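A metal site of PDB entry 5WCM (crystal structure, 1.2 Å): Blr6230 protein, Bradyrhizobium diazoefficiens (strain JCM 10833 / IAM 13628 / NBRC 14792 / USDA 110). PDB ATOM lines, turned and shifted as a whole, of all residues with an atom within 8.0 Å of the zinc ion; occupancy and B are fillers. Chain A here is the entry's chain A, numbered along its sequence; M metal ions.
OE2 of Glu 127 is bound to the zinc ion, at 2.0 Å. A ring nitrogen (ND1) of His 141 is bound to the zinc ion (2.0 Å). The zinc ion is bound by NZ of Lys 198 (2.1 Å). Slightly farther from the zinc ion lies the side-chain carboxylate (OE1) of Glu 127 (2.8 Å).
Within 4 Å of the zinc ion: Glu 127, His 141 and Lys 198.
OE1 of Glu 127 sits at hydrogen-bond distance from N of Ala 142, at 2.8 Å. O of Ser 152 is in hydrogen-bond range of N of His 141 (2.8 Å). A ring nitrogen (NE2) of His 141 lies within hydrogen-bond range of the side-chain carboxylate (OE2) of Glu 154 (2.7 Å).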
ATOM      1  N   LYS A 126       6.840 -26.372 -16.386  1.00  0.00           N
ATOM      2  CA  LYS A 126       8.211 -25.898 -16.624  1.00  0.00           C
ATOM      3  C   LYS A 126       8.252 -24.408 -16.364  1.00  0.00           C
ATOM      4  O   LYS A 126       7.218 -23.762 -16.195  1.00  0.00           O
ATOM      5  CB  LYS A 126       8.683 -26.200 -18.040  1.00  0.00           C
ATOM      6  CG  LYS A 126       7.750 -25.693 -19.123  1.00  0.00           C
ATOM      7  N   GLU A 127       9.472 -23.868 -16.320  1.00  0.00           N
ATOM      8  CA  GLU A 127       9.723 -22.435 -16.107  1.00  0.00           C
ATOM      9  C   GLU A 127       8.787 -21.588 -16.965  1.00  0.00           C
ATOM     10  O   GLU A 127       8.707 -21.755 -18.190  1.00  0.00           O
ATOM     11  CB  GLU A 127      11.184 -22.070 -16.443  1.00  0.00           C
ATOM     12  CG  GLU A 127      11.513 -20.571 -16.489  1.00  0.00           C
ATOM     13  CD  GLU A 127      11.494 -19.865 -15.142  1.00  0.00           C
ATOM     14  OE1 GLU A 127      11.661 -20.531 -14.104  1.00  0.00           O
ATOM     15  OE2 GLU A 127      11.347 -18.620 -15.133  1.00  0.00           O
ATOM     16  N   GLY A 128       8.103 -20.662 -16.311  1.00  0.00           N
ATOM     17  CA  GLY A 128       7.216 -19.702 -16.979  1.00  0.00           C
ATOM     18  C   GLY A 128       5.789 -20.141 -17.235  1.00  0.00           C
ATOM     19  O   GLY A 128       4.957 -19.305 -17.663  1.00  0.00           O
ATOM     20  N   THR A 139       2.502 -18.301 -11.561  1.00  0.00           N
ATOM     21  CA  THR A 139       3.548 -18.578 -12.534  1.00  0.00           C
ATOM     22  C   THR A 139       4.595 -19.491 -11.925  1.00  0.00           C
ATOM     23  O   THR A 139       5.114 -19.212 -10.846  1.00  0.00           O
ATOM     24  CB  THR A 139       4.212 -17.294 -13.054  1.00  0.00           C
ATOM     25  OG1 THR A 139       3.191 -16.473 -13.631  1.00  0.00           O
ATOM     26  CG2 THR A 139       5.255 -17.584 -14.123  1.00  0.00           C
ATOM     27  N   ALA A 140       4.902 -20.563 -12.633  1.00  0.00           N
ATOM     28  CA  ALA A 140       5.917 -21.531 -12.200  1.00  0.00           C
ATOM     29  C   ALA A 140       7.313 -21.014 -12.467  1.00  0.00           C
ATOM     30  O   ALA A 140       7.587 -20.527 -13.582  1.00  0.00           O
ATOM     31  CB  ALA A 140       5.750 -22.859 -12.903  1.00  0.00           C
ATOM     32  N   HIS A 141       8.194 -21.154 -11.491  1.00  0.00           N
ATOM     33  CA  HIS A 141       9.630 -20.914 -11.684  1.00  0.00           C
ATOM     34  C   HIS A 141      10.410 -22.182 -11.321  1.00  0.00           C
ATOM     35  O   HIS A 141      10.228 -22.722 -10.222  1.00  0.00           O
ATOM     36  CB  HIS A 141      10.116 -19.741 -10.858  1.00  0.00           C
ATOM     37  CG  HIS A 141       9.509 -18.443 -11.256  1.00  0.00           C
ATOM     38  ND1 HIS A 141      10.083 -17.612 -12.203  1.00  0.00           N
ATOM     39  CD2 HIS A 141       8.370 -17.845 -10.836  1.00  0.00           C
ATOM     40  CE1 HIS A 141       9.293 -16.557 -12.346  1.00  0.00           C
ATOM     41  NE2 HIS A 141       8.262 -16.674 -11.536  1.00  0.00           N
ATOM     42  N   ALA A 142      11.243 -22.642 -12.236  1.00  0.00           N
ATOM     43  CA  ALA A 142      12.078 -23.795 -11.991  1.00  0.00           C
ATOM     44  C   ALA A 142      13.245 -23.393 -11.075  1.00  0.00           C
ATOM     45  O   ALA A 142      14.149 -22.659 -11.492  1.00  0.00           O
ATOM     46  CB  ALA A 142      12.592 -24.382 -13.291  1.00  0.00           C
ATOM     47  N   THR A 143      13.193 -23.866  -9.835  1.00  0.00           N
ATOM     48  CA  THR A 143      14.221 -23.592  -8.833  1.00  0.00           C
ATOM     49  C   THR A 143      14.701 -24.920  -8.216  1.00  0.00           C
ATOM     50  O   THR A 143      14.582 -25.129  -7.007  1.00  0.00           O
ATOM     51  CB  THR A 143      13.681 -22.642  -7.751  1.00  0.00           C
ATOM     52  OG1 THR A 143      12.409 -23.110  -7.294  1.00  0.00           O
ATOM     53  CG2 THR A 143      13.455 -21.232  -8.304  1.00  0.00           C
ATOM     54  N   SER A 152       9.088 -22.953  -7.544  1.00  0.00           N
ATOM     55  CA  SER A 152       8.663 -21.776  -6.801  1.00  0.00           C
ATOM     56  C   SER A 152       7.542 -21.091  -7.563  1.00  0.00           C
ATOM     57  O   SER A 152       7.613 -20.903  -8.787  1.00  0.00           O
ATOM     58  CB  SER A 152       9.850 -20.832  -6.569  1.00  0.00           C
ATOM     59  OG  SER A 152      10.874 -21.450  -5.809  1.00  0.00           O
ATOM     60  N   GLU A 154       4.918 -17.952  -8.306  1.00  0.00           N
ATOM     61  CA  GLU A 154       4.755 -16.497  -8.249  1.00  0.00           C
ATOM     62  C   GLU A 154       3.276 -16.140  -8.423  1.00  0.00           C
ATOM     63  O   GLU A 154       2.631 -16.669  -9.318  1.00  0.00           O
ATOM     64  CB  GLU A 154       5.609 -15.866  -9.361  1.00  0.00           C
ATOM     65  CG  GLU A 154       5.434 -14.379  -9.643  1.00  0.00           C
ATOM     66  CD  GLU A 154       6.409 -13.890 -10.696  1.00  0.00           C
ATOM     67  OE1 GLU A 154       7.050 -12.850 -10.468  1.00  0.00           O
ATOM     68  OE2 GLU A 154       6.546 -14.567 -11.743  1.00  0.00           O
ATOM     69  N   LEU A 167       6.182 -14.843  -3.728  1.00  0.00           N
ATOM     70  CA  LEU A 167       6.795 -16.117  -4.156  1.00  0.00           C
ATOM     71  C   LEU A 167       6.632 -17.171  -3.076  1.00  0.00           C
ATOM     72  O   LEU A 167       7.108 -17.015  -1.960  1.00  0.00           O
ATOM     73  CB  LEU A 167       8.285 -15.965  -4.478  1.00  0.00           C
ATOM     74  CG  LEU A 167       8.887 -17.161  -5.214  1.00  0.00           C
ATOM     75  CD1 LEU A 167       8.432 -17.199  -6.663  1.00  0.00           C
ATOM     76  CD2 LEU A 167      10.403 -17.149  -5.124  1.00  0.00           C
ATOM     77  N   LYS A 198      19.274 -17.276  -9.101  1.00  0.00           N
ATOM     78  CA  LYS A 198      17.964 -16.948  -9.659  1.00  0.00           C
ATOM     79  C   LYS A 198      17.075 -16.269  -8.598  1.00  0.00           C
ATOM     80  O   LYS A 198      16.447 -15.245  -8.881  1.00  0.00           O
ATOM     81  CB  LYS A 198      17.271 -18.218 -10.166  1.00  0.00           C
ATOM     82  CG  LYS A 198      15.870 -17.995 -10.688  1.00  0.00           C
ATOM     83  CD  LYS A 198      15.302 -19.305 -11.196  1.00  0.00           C
ATOM     84  CE  LYS A 198      13.832 -19.226 -11.546  1.00  0.00           C
ATOM     85  NZ  LYS A 198      13.583 -18.216 -12.599  1.00  0.00           N
ATOM     86  N   MET A 202      15.099 -12.080  -8.434  1.00  0.00           N
ATOM     87  CA  MET A 202      13.656 -11.914  -8.546  1.00  0.00           C
ATOM     88  C   MET A 202      13.213 -10.732  -7.700  1.00  0.00           C
ATOM     89  O   MET A 202      13.770 -10.488  -6.629  1.00  0.00           O
ATOM     90  CB  MET A 202      12.925 -13.137  -8.081  1.00  0.00           C
ATOM     91  CG  MET A 202      12.953 -14.284  -9.045  1.00  0.00           C
ATOM     92  SD  MET A 202      11.996 -15.554  -8.236  1.00  0.00           S
ATOM     93  CE  MET A 202      12.138 -16.863  -9.425  1.00  0.00           C
HETATM   94 ZN    ZN M   1      11.715 -17.834 -13.370  1.00  0.00          ZN
